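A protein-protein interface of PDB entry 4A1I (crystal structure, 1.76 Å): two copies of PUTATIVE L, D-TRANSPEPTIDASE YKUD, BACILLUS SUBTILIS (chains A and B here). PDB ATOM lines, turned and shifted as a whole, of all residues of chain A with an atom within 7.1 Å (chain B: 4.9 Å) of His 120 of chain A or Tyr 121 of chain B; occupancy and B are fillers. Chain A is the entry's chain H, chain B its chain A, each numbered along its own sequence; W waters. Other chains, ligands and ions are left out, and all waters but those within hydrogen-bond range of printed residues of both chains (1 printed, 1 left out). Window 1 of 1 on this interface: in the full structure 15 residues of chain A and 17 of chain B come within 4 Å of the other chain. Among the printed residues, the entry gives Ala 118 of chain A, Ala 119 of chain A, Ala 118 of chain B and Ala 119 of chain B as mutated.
NH2 of Arg 21 of chain B sits at hydrogen-bond distance from O of Tyr 121 of chain B (3.0 Å).
NE1 of Trp 113 of chain B lies within hydrogen-bond range of OG of Ser 115 of chain B (2.7 Å).
The backbone NH (N) of Leu 116 of chain B sits at hydrogen-bond distance from the backbone carbonyl oxygen (O) of Tyr 121 of chain B, at 2.9 Å.
N of Ala 119 of chain A lies within hydrogen-bond range of OD1 of Asp 19 of chain A (2.9 Å).
The backbone carbonyl oxygen of Tyr 121 of chain A lies within hydrogen-bond range of the guanidinium group of Arg 21 of chain A (3.0 Å).
N of Leu 116 of chain A sits at hydrogen-bond distance from O of Tyr 121 of chain A (2.9 Å).
Among the printed residues, merely in contact across the chains: Phe 109 of chain A with Lys 138 of chain B, Trp 113 of chain A with Lys 138 of chain B, Ala 119 of chain A with Tyr 121 of chain B, His 120 of chain A with His 120 of chain B, His 120 of chain A with Tyr 121 of chain B, His 120 of chain A with Lys 138 of chain B, Tyr 121 of chain A with Ala 119 of chain B, Tyr 121 of chain A with His 120 of chain B, Lys 138 of chain A with Trp 113 of chain B and Lys 138 of chain A with His 120 of chain B.
Of chain B, only His 120, Tyr 121 and Lys 138 come within 4 Å of His 120 of chain A.
Of chain A, only Ala 119 (3.2 Å) and His 120 (3.6 Å) come within 4 Å of Tyr 121 of chain B.
Of the printed residues of chain A, Trp 113 of chain B touches Lys 138 (3.7 Å).
Printed residues of chain A within 4 Å of Ala 119 of chain B: Tyr 121.
The nearest residue of chain B that does not touch His 120 of chain A is Cys 140 of chain B (4.1 Å).
Of the 16 printed residues of chain B, 5 touch a printed residue of chain A.
Printed residues of chain B that touch a printed residue of chain A: Trp 113, Ala 119, His 120, Tyr 121 and Lys 138.
Hydrophobic or aromatic side chains of chain B within 4 Å of the printed part of chain A: Trp 113, Ala 119, His 120 and Tyr 121.
Among the printed residues, 10 pairs touch across the chains.
Trp 113 of chain A touches Lys 138 of chain B, and with the chains exchanged Lys 138 of chain A touches Trp 113 of chain B.
Ala 119 of chain A touches Tyr 121 of chain B, and with the chains exchanged Tyr 121 of chain A touches Ala 119 of chain B.
His 120 of chain B touches its own counterpart, His 120 of chain A.
His 120 of chain A touches Lys 138 of chain B, and with the chains exchanged Lys 138 of chain A touches His 120 of chain B.
Of the 10 pairs that touch across the chains among the printed residues, 9 have their exchanged pair printed and touching as well.
Water W1 bridges the backbone carbonyl oxygen of Lys 138 of chain B and the backbone NH of His 120 of chain A.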
ATOM      1  N   ALA A  18      -2.848  -6.786 -23.590  1.00  0.00           N
ATOM      2  CA  ALA A  18      -1.582  -7.071 -24.256  1.00  0.00           C
ATOM      3  C   ALA A  18      -1.327  -8.574 -24.391  1.00  0.00           C
ATOM      4  O   ALA A  18      -0.779  -9.026 -25.395  1.00  0.00           O
ATOM      5  CB  ALA A  18      -0.426  -6.395 -23.516  1.00  0.00           C
ATOM      6  N   ASP A  19      -1.710  -9.348 -23.380  1.00  0.00           N
ATOM      7  CA  ASP A  19      -1.541 -10.793 -23.458  1.00  0.00           C
ATOM      8  C   ASP A  19      -2.387 -11.380 -24.581  1.00  0.00           C
ATOM      9  O   ASP A  19      -1.951 -12.290 -25.290  1.00  0.00           O
ATOM     10  CB  ASP A  19      -1.927 -11.463 -22.140  1.00  0.00           C
ATOM     11  CG  ASP A  19      -0.812 -11.426 -21.118  1.00  0.00           C
ATOM     12  OD1 ASP A  19       0.336 -11.071 -21.483  1.00  0.00           O
ATOM     13  OD2 ASP A  19      -1.079 -11.775 -19.946  1.00  0.00           O
ATOM     14  N   ARG A  21      -3.796  -9.719 -27.185  1.00  0.00           N
ATOM     15  CA  ARG A  21      -3.702  -8.960 -28.437  1.00  0.00           C
ATOM     16  C   ARG A  21      -5.037  -8.358 -28.858  1.00  0.00           C
ATOM     17  O   ARG A  21      -5.466  -8.513 -30.001  1.00  0.00           O
ATOM     18  CB  ARG A  21      -3.148  -9.834 -29.571  1.00  0.00           C
ATOM     19  CG  ARG A  21      -1.886 -10.615 -29.224  1.00  0.00           C
ATOM     20  CD  ARG A  21      -0.689  -9.716 -28.856  1.00  0.00           C
ATOM     21  NE  ARG A  21       0.566 -10.461 -29.003  1.00  0.00           N
ATOM     22  CZ  ARG A  21       0.984 -11.411 -28.163  1.00  0.00           C
ATOM     23  NH1 ARG A  21       0.270 -11.723 -27.087  1.00  0.00           N
ATOM     24  NH2 ARG A  21       2.124 -12.052 -28.396  1.00  0.00           N
ATOM     25  N   PHE A 109      11.931 -13.241 -38.104  1.00  0.00           N
ATOM     26  CA  PHE A 109      10.671 -13.921 -37.817  1.00  0.00           C
ATOM     27  C   PHE A 109      10.249 -14.906 -38.905  1.00  0.00           C
ATOM     28  O   PHE A 109       9.353 -15.721 -38.693  1.00  0.00           O
ATOM     29  CB  PHE A 109       9.565 -12.903 -37.555  1.00  0.00           C
ATOM     30  CG  PHE A 109       9.922 -11.901 -36.505  1.00  0.00           C
ATOM     31  CD1 PHE A 109      10.218 -12.313 -35.217  1.00  0.00           C
ATOM     32  CD2 PHE A 109      10.001 -10.553 -36.811  1.00  0.00           C
ATOM     33  CE1 PHE A 109      10.565 -11.394 -34.242  1.00  0.00           C
ATOM     34  CE2 PHE A 109      10.344  -9.628 -35.840  1.00  0.00           C
ATOM     35  CZ  PHE A 109      10.629 -10.051 -34.557  1.00  0.00           C
ATOM     36  N   TRP A 113       4.404 -15.434 -38.156  1.00  0.00           N
ATOM     37  CA  TRP A 113       4.408 -15.218 -36.723  1.00  0.00           C
ATOM     38  C   TRP A 113       3.053 -15.639 -36.186  1.00  0.00           C
ATOM     39  O   TRP A 113       2.022 -15.199 -36.686  1.00  0.00           O
ATOM     40  CB  TRP A 113       4.660 -13.750 -36.391  1.00  0.00           C
ATOM     41  CG  TRP A 113       4.372 -13.437 -34.958  1.00  0.00           C
ATOM     42  CD1 TRP A 113       3.144 -13.268 -34.395  1.00  0.00           C
ATOM     43  CD2 TRP A 113       5.327 -13.272 -33.899  1.00  0.00           C
ATOM     44  NE1 TRP A 113       3.269 -13.001 -33.053  1.00  0.00           N
ATOM     45  CE2 TRP A 113       4.600 -12.998 -32.722  1.00  0.00           C
ATOM     46  CE3 TRP A 113       6.723 -13.322 -33.832  1.00  0.00           C
ATOM     47  CZ2 TRP A 113       5.219 -12.776 -31.489  1.00  0.00           C
ATOM     48  CZ3 TRP A 113       7.339 -13.103 -32.603  1.00  0.00           C
ATOM     49  CH2 TRP A 113       6.586 -12.830 -31.451  1.00  0.00           C
ATOM     50  N   LEU A 116       1.331 -15.980 -29.181  1.00  0.00           N
ATOM     51  CA  LEU A 116       0.887 -16.740 -28.018  1.00  0.00           C
ATOM     52  C   LEU A 116       0.260 -15.780 -27.002  1.00  0.00           C
ATOM     53  O   LEU A 116       0.549 -14.573 -27.008  1.00  0.00           O
ATOM     54  CB  LEU A 116       2.060 -17.508 -27.391  1.00  0.00           C
ATOM     55  CG  LEU A 116       2.603 -18.675 -28.225  1.00  0.00           C
ATOM     56  CD1 LEU A 116       3.929 -19.175 -27.672  1.00  0.00           C
ATOM     57  CD2 LEU A 116       1.585 -19.798 -28.258  1.00  0.00           C
ATOM     58  N   SER A 117      -0.594 -16.315 -26.135  1.00  0.00           N
ATOM     59  CA  SER A 117      -1.318 -15.496 -25.153  1.00  0.00           C
ATOM     60  C   SER A 117      -0.455 -14.988 -23.993  1.00  0.00           C
ATOM     61  O   SER A 117      -0.954 -14.792 -22.884  1.00  0.00           O
ATOM     62  CB  SER A 117      -2.529 -16.258 -24.608  1.00  0.00           C
ATOM     63  OG  SER A 117      -2.142 -17.510 -24.064  1.00  0.00           O
ATOM     64  N   ALA A 118       0.836 -14.796 -24.248  1.00  0.00           N
ATOM     65  CA  ALA A 118       1.723 -14.075 -23.337  1.00  0.00           C
ATOM     66  C   ALA A 118       2.352 -12.913 -24.113  1.00  0.00           C
ATOM     67  O   ALA A 118       2.887 -13.111 -25.198  1.00  0.00           O
ATOM     68  CB  ALA A 118       2.803 -15.002 -22.787  1.00  0.00           C
ATOM     69  N   ALA A 119       2.260 -11.701 -23.569  1.00  0.00           N
ATOM     70  CA  ALA A 119       2.729 -10.507 -24.274  1.00  0.00           C
ATOM     71  C   ALA A 119       4.153 -10.654 -24.815  1.00  0.00           C
ATOM     72  O   ALA A 119       5.075 -10.983 -24.072  1.00  0.00           O
ATOM     73  CB  ALA A 119       2.620  -9.282 -23.369  1.00  0.00           C
ATOM     74  N   HIS A 120       4.307 -10.412 -26.118  1.00  0.00           N
ATOM     75  CA  HIS A 120       5.598 -10.439 -26.815  1.00  0.00           C
ATOM     76  C   HIS A 120       6.054 -11.839 -27.232  1.00  0.00           C
ATOM     77  O   HIS A 120       7.047 -11.974 -27.956  1.00  0.00           O
ATOM     78  CB  HIS A 120       6.704  -9.745 -26.010  1.00  0.00           C
ATOM     79  CG  HIS A 120       7.758  -9.110 -26.865  1.00  0.00           C
ATOM     80  ND1 HIS A 120       8.225  -9.687 -28.026  1.00  0.00           N
ATOM     81  CD2 HIS A 120       8.406  -7.926 -26.747  1.00  0.00           C
ATOM     82  CE1 HIS A 120       9.134  -8.900 -28.573  1.00  0.00           C
ATOM     83  NE2 HIS A 120       9.256  -7.822 -27.820  1.00  0.00           N
ATOM     84  N   TYR A 121       5.332 -12.867 -26.792  1.00  0.00           N
ATOM     85  CA  TYR A 121       5.734 -14.243 -27.087  1.00  0.00           C
ATOM     86  C   TYR A 121       4.954 -14.830 -28.244  1.00  0.00           C
ATOM     87  O   TYR A 121       3.773 -14.542 -28.433  1.00  0.00           O
ATOM     88  CB  TYR A 121       5.600 -15.141 -25.858  1.00  0.00           C
ATOM     89  CG  TYR A 121       6.662 -14.853 -24.828  1.00  0.00           C
ATOM     90  CD1 TYR A 121       6.510 -13.813 -23.927  1.00  0.00           C
ATOM     91  CD2 TYR A 121       7.829 -15.605 -24.777  1.00  0.00           C
ATOM     92  CE1 TYR A 121       7.487 -13.529 -22.994  1.00  0.00           C
ATOM     93  CE2 TYR A 121       8.814 -15.328 -23.844  1.00  0.00           C
ATOM     94  CZ  TYR A 121       8.634 -14.291 -22.960  1.00  0.00           C
ATOM     95  OH  TYR A 121       9.605 -14.007 -22.033  1.00  0.00           O
ATOM     96  N   GLY A 122       5.624 -15.678 -29.010  1.00  0.00           N
ATOM     97  CA  GLY A 122       4.972 -16.323 -30.123  1.00  0.00           C
ATOM     98  C   GLY A 122       5.754 -17.507 -30.635  1.00  0.00           C
ATOM     99  O   GLY A 122       6.809 -17.857 -30.099  1.00  0.00           O
ATOM    100  N   HIS A 124       7.377 -18.572 -34.252  1.00  0.00           N
ATOM    101  CA  HIS A 124       7.681 -18.000 -35.554  1.00  0.00           C
ATOM    102  C   HIS A 124       8.758 -18.755 -36.317  1.00  0.00           C
ATOM    103  O   HIS A 124       9.352 -19.713 -35.806  1.00  0.00           O
ATOM    104  CB  HIS A 124       8.026 -16.497 -35.451  1.00  0.00           C
ATOM    105  CG  HIS A 124       9.239 -16.193 -34.622  1.00  0.00           C
ATOM    106  ND1 HIS A 124      10.525 -16.317 -35.108  1.00  0.00           N
ATOM    107  CD2 HIS A 124       9.360 -15.747 -33.349  1.00  0.00           C
ATOM    108  CE1 HIS A 124      11.383 -15.963 -34.167  1.00  0.00           C
ATOM    109  NE2 HIS A 124      10.703 -15.616 -33.090  1.00  0.00           N
ATOM    110  N   LYS A 138      15.232 -15.326 -27.399  1.00  0.00           N
ATOM    111  CA  LYS A 138      14.868 -14.423 -26.313  1.00  0.00           C
ATOM    112  C   LYS A 138      13.682 -14.978 -25.528  1.00  0.00           C
ATOM    113  O   LYS A 138      13.277 -14.405 -24.518  1.00  0.00           O
ATOM    114  CB  LYS A 138      14.534 -13.032 -26.855  1.00  0.00           C
ATOM    115  CG  LYS A 138      15.743 -12.205 -27.263  1.00  0.00           C
ATOM    116  CD  LYS A 138      15.312 -10.796 -27.670  1.00  0.00           C
ATOM    117  CE  LYS A 138      16.505  -9.907 -28.000  1.00  0.00           C
ATOM    118  NZ  LYS A 138      17.397  -9.687 -26.831  1.00  0.00           N
ATOM    119  N   GLY A 139      13.133 -16.100 -25.992  1.00  0.00           N
ATOM    120  CA  GLY A 139      11.987 -16.704 -25.335  1.00  0.00           C
ATOM    121  C   GLY A 139      10.944 -17.280 -26.279  1.00  0.00           C
ATOM    122  O   GLY A 139      10.157 -18.124 -25.877  1.00  0.00           O
ATOM    123  N   CYS A 140      10.908 -16.813 -27.525  1.00  0.00           N
ATOM    124  CA  CYS A 140       9.967 -17.366 -28.497  1.00  0.00           C
ATOM    125  C   CYS A 140      10.362 -18.775 -28.892  1.00  0.00           C
ATOM    126  O   CYS A 140      11.507 -19.187 -28.723  1.00  0.00           O
ATOM    127  CB  CYS A 140       9.904 -16.523 -29.770  1.00  0.00           C
ATOM    128  SG  CYS A 140       8.838 -15.061 -29.664  1.00  0.00           S
ATOM    129  N   ARG B  21      16.291 -11.737 -15.499  1.00  0.00           N
ATOM    130  CA  ARG B  21      17.394 -12.301 -16.286  1.00  0.00           C
ATOM    131  C   ARG B  21      18.447 -12.969 -15.405  1.00  0.00           C
ATOM    132  O   ARG B  21      19.652 -12.739 -15.563  1.00  0.00           O
ATOM    133  CB  ARG B  21      18.043 -11.234 -17.180  1.00  0.00           C
ATOM    134  CG  ARG B  21      17.062 -10.318 -17.932  1.00  0.00           C
ATOM    135  CD  ARG B  21      16.129 -11.089 -18.879  1.00  0.00           C
ATOM    136  NE  ARG B  21      15.627 -10.237 -19.956  1.00  0.00           N
ATOM    137  CZ  ARG B  21      14.609  -9.385 -19.836  1.00  0.00           C
ATOM    138  NH1 ARG B  21      13.960  -9.269 -18.679  1.00  0.00           N
ATOM    139  NH2 ARG B  21      14.241  -8.645 -20.875  1.00  0.00           N
ATOM    140  N   GLN B  90       1.233  -3.460 -27.075  1.00  0.00           N
ATOM    141  CA  GLN B  90       1.749  -2.242 -26.474  1.00  0.00           C
ATOM    142  C   GLN B  90       2.954  -2.431 -25.572  1.00  0.00           C
ATOM    143  O   GLN B  90       3.228  -3.523 -25.084  1.00  0.00           O
ATOM    144  CB  GLN B  90       0.648  -1.531 -25.694  1.00  0.00           C
ATOM    145  CG  GLN B  90      -0.321  -0.768 -26.566  1.00  0.00           C
ATOM    146  CD  GLN B  90      -0.993   0.341 -25.801  1.00  0.00           C
ATOM    147  OE1 GLN B  90      -1.639   0.093 -24.784  1.00  0.00           O
ATOM    148  NE2 GLN B  90      -0.815   1.580 -26.262  1.00  0.00           N
ATOM    149  N   PRO B  92       4.457  -2.175 -22.087  1.00  0.00           N
ATOM    150  CA  PRO B  92       3.824  -2.276 -20.768  1.00  0.00           C
ATOM    151  C   PRO B  92       4.089  -1.035 -19.919  1.00  0.00           C
ATOM    152  O   PRO B  92       5.134  -0.403 -20.053  1.00  0.00           O
ATOM    153  CB  PRO B  92       4.505  -3.497 -20.147  1.00  0.00           C
ATOM    154  CG  PRO B  92       5.823  -3.579 -20.823  1.00  0.00           C
ATOM    155  CD  PRO B  92       5.595  -3.100 -22.232  1.00  0.00           C
ATOM    156  N   TRP B 113      21.235  -3.156 -26.702  1.00  0.00           N
ATOM    157  CA  TRP B 113      20.049  -3.687 -26.047  1.00  0.00           C
ATOM    158  C   TRP B 113      20.189  -3.470 -24.544  1.00  0.00           C
ATOM    159  O   TRP B 113      21.210  -3.820 -23.957  1.00  0.00           O
ATOM    160  CB  TRP B 113      19.888  -5.185 -26.342  1.00  0.00           C
ATOM    161  CG  TRP B 113      18.834  -5.849 -25.488  1.00  0.00           C
ATOM    162  CD1 TRP B 113      18.989  -6.319 -24.215  1.00  0.00           C
ATOM    163  CD2 TRP B 113      17.468  -6.109 -25.847  1.00  0.00           C
ATOM    164  NE1 TRP B 113      17.808  -6.855 -23.759  1.00  0.00           N
ATOM    165  CE2 TRP B 113      16.859  -6.739 -24.741  1.00  0.00           C
ATOM    166  CE3 TRP B 113      16.702  -5.871 -26.996  1.00  0.00           C
ATOM    167  CZ2 TRP B 113      15.516  -7.129 -24.746  1.00  0.00           C
ATOM    168  CZ3 TRP B 113      15.367  -6.266 -27.001  1.00  0.00           C
ATOM    169  CH2 TRP B 113      14.790  -6.884 -25.881  1.00  0.00           C
ATOM    170  N   LEU B 114      19.172  -2.868 -23.935  1.00  0.00           N
ATOM    171  CA  LEU B 114      19.088  -2.779 -22.484  1.00  0.00           C
ATOM    172  C   LEU B 114      17.860  -3.569 -22.033  1.00  0.00           C
ATOM    173  O   LEU B 114      16.735  -3.230 -22.391  1.00  0.00           O
ATOM    174  CB  LEU B 114      18.964  -1.320 -22.033  1.00  0.00           C
ATOM    175  CG  LEU B 114      19.886  -0.290 -22.696  1.00  0.00           C
ATOM    176  CD1 LEU B 114      19.543   1.132 -22.251  1.00  0.00           C
ATOM    177  CD2 LEU B 114      21.330  -0.605 -22.402  1.00  0.00           C
ATOM    178  N   SER B 115      18.072  -4.629 -21.257  1.00  0.00           N
ATOM    179  CA  SER B 115      16.949  -5.395 -20.729  1.00  0.00           C
ATOM    180  C   SER B 115      16.190  -4.618 -19.673  1.00  0.00           C
ATOM    181  O   SER B 115      16.792  -3.985 -18.800  1.00  0.00           O
ATOM    182  CB  SER B 115      17.420  -6.715 -20.120  1.00  0.00           C
ATOM    183  OG  SER B 115      17.920  -7.570 -21.121  1.00  0.00           O
ATOM    184  N   LEU B 116      14.864  -4.678 -19.753  1.00  0.00           N
ATOM    185  CA  LEU B 116      14.013  -4.159 -18.690  1.00  0.00           C
ATOM    186  C   LEU B 116      13.531  -5.308 -17.834  1.00  0.00           C
ATOM    187  O   LEU B 116      13.548  -6.464 -18.263  1.00  0.00           O
ATOM    188  CB  LEU B 116      12.809  -3.416 -19.273  1.00  0.00           C
ATOM    189  CG  LEU B 116      13.121  -2.107 -19.996  1.00  0.00           C
ATOM    190  CD1 LEU B 116      11.898  -1.603 -20.751  1.00  0.00           C
ATOM    191  CD2 LEU B 116      13.613  -1.064 -19.001  1.00  0.00           C
ATOM    192  N   ALA B 118      10.972  -6.753 -17.310  1.00  0.00           N
ATOM    193  CA  ALA B 118       9.847  -7.575 -17.749  1.00  0.00           C
ATOM    194  C   ALA B 118      10.356  -8.511 -18.840  1.00  0.00           C
ATOM    195  O   ALA B 118      11.016  -8.072 -19.777  1.00  0.00           O
ATOM    196  CB  ALA B 118       8.704  -6.707 -18.269  1.00  0.00           C
ATOM    197  N   ALA B 119      10.082  -9.804 -18.707  1.00  0.00           N
ATOM    198  CA  ALA B 119      10.644 -10.774 -19.647  1.00  0.00           C
ATOM    199  C   ALA B 119      10.343 -10.385 -21.096  1.00  0.00           C
ATOM    200  O   ALA B 119       9.199 -10.067 -21.437  1.00  0.00           O
ATOM    201  CB  ALA B 119      10.128 -12.169 -19.341  1.00  0.00           C
ATOM    202  N   HIS B 120      11.393 -10.419 -21.923  1.00  0.00           N
ATOM    203  CA  HIS B 120      11.358 -10.105 -23.354  1.00  0.00           C
ATOM    204  C   HIS B 120      11.372  -8.608 -23.686  1.00  0.00           C
ATOM    205  O   HIS B 120      11.521  -8.235 -24.846  1.00  0.00           O
ATOM    206  CB  HIS B 120      10.203 -10.824 -24.073  1.00  0.00           C
ATOM    207  CG  HIS B 120      10.537 -11.241 -25.473  1.00  0.00           C
ATOM    208  ND1 HIS B 120      11.330 -10.481 -26.304  1.00  0.00           N
ATOM    209  CD2 HIS B 120      10.205 -12.348 -26.177  1.00  0.00           C
ATOM    210  CE1 HIS B 120      11.457 -11.092 -27.470  1.00  0.00           C
ATOM    211  NE2 HIS B 120      10.786 -12.228 -27.415  1.00  0.00           N
ATOM    212  N   TYR B 121      11.242  -7.754 -22.675  1.00  0.00           N
ATOM    213  CA  TYR B 121      11.188  -6.317 -22.936  1.00  0.00           C
ATOM    214  C   TYR B 121      12.505  -5.615 -22.688  1.00  0.00           C
ATOM    215  O   TYR B 121      13.284  -6.009 -21.824  1.00  0.00           O
ATOM    216  CB  TYR B 121      10.076  -5.651 -22.126  1.00  0.00           C
ATOM    217  CG  TYR B 121       8.719  -6.066 -22.617  1.00  0.00           C
ATOM    218  CD1 TYR B 121       8.085  -5.363 -23.637  1.00  0.00           C
ATOM    219  CD2 TYR B 121       8.083  -7.179 -22.091  1.00  0.00           C
ATOM    220  CE1 TYR B 121       6.847  -5.755 -24.108  1.00  0.00           C
ATOM    221  CE2 TYR B 121       6.844  -7.577 -22.555  1.00  0.00           C
ATOM    222  CZ  TYR B 121       6.234  -6.861 -23.563  1.00  0.00           C
ATOM    223  OH  TYR B 121       5.001  -7.257 -24.031  1.00  0.00           O
ATOM    224  N   GLY B 122      12.736  -4.555 -23.449  1.00  0.00           N
ATOM    225  CA  GLY B 122      13.913  -3.736 -23.249  1.00  0.00           C
ATOM    226  C   GLY B 122      13.823  -2.417 -23.985  1.00  0.00           C
ATOM    227  O   GLY B 122      12.805  -2.099 -24.610  1.00  0.00           O
ATOM    228  N   ILE B 123      14.901  -1.649 -23.878  1.00  0.00           N
ATOM    229  CA  ILE B 123      15.121  -0.453 -24.664  1.00  0.00           C
ATOM    230  C   ILE B 123      16.250  -0.798 -25.623  1.00  0.00           C
ATOM    231  O   ILE B 123      17.291  -1.288 -25.198  1.00  0.00           O
ATOM    232  CB  ILE B 123      15.582   0.694 -23.758  1.00  0.00           C
ATOM    233  CG1 ILE B 123      14.551   0.946 -22.655  1.00  0.00           C
ATOM    234  CG2 ILE B 123      15.856   1.959 -24.576  1.00  0.00           C
ATOM    235  CD1 ILE B 123      15.084   1.788 -21.497  1.00  0.00           C
ATOM    236  N   LYS B 138       6.807  -4.477 -31.238  1.00  0.00           N
ATOM    237  CA  LYS B 138       6.150  -5.589 -30.555  1.00  0.00           C
ATOM    238  C   LYS B 138       5.959  -5.321 -29.068  1.00  0.00           C
ATOM    239  O   LYS B 138       5.313  -6.103 -28.374  1.00  0.00           O
ATOM    240  CB  LYS B 138       6.960  -6.879 -30.714  1.00  0.00           C
ATOM    241  CG  LYS B 138       6.815  -7.560 -32.060  1.00  0.00           C
ATOM    242  CD  LYS B 138       7.438  -8.947 -32.011  1.00  0.00           C
ATOM    243  CE  LYS B 138       7.295  -9.671 -33.337  1.00  0.00           C
ATOM    244  NZ  LYS B 138       5.875 -10.002 -33.658  1.00  0.00           N
ATOM    245  N   GLY B 139       6.544  -4.238 -28.571  1.00  0.00           N
ATOM    246  CA  GLY B 139       6.387  -3.878 -27.173  1.00  0.00           C
ATOM    247  C   GLY B 139       7.578  -3.150 -26.576  1.00  0.00           C
ATOM    248  O   GLY B 139       7.440  -2.441 -25.582  1.00  0.00           O
ATOM    249  N   CYS B 140       8.747  -3.320 -27.187  1.00  0.00           N
ATOM    250  CA  CYS B 140       9.960  -2.663 -26.724  1.00  0.00           C
ATOM    251  C   CYS B 140       9.948  -1.176 -26.993  1.00  0.00           C
ATOM    252  O   CYS B 140       9.172  -0.672 -27.807  1.00  0.00           O
ATOM    253  CB  CYS B 140      11.196  -3.253 -27.403  1.00  0.00           C
ATOM    254  SG  CYS B 140      11.773  -4.767 -26.644  1.00  0.00           S
HETATM  255  O   HOH W   1       3.904  -8.510 -28.701  1.00  0.00           O
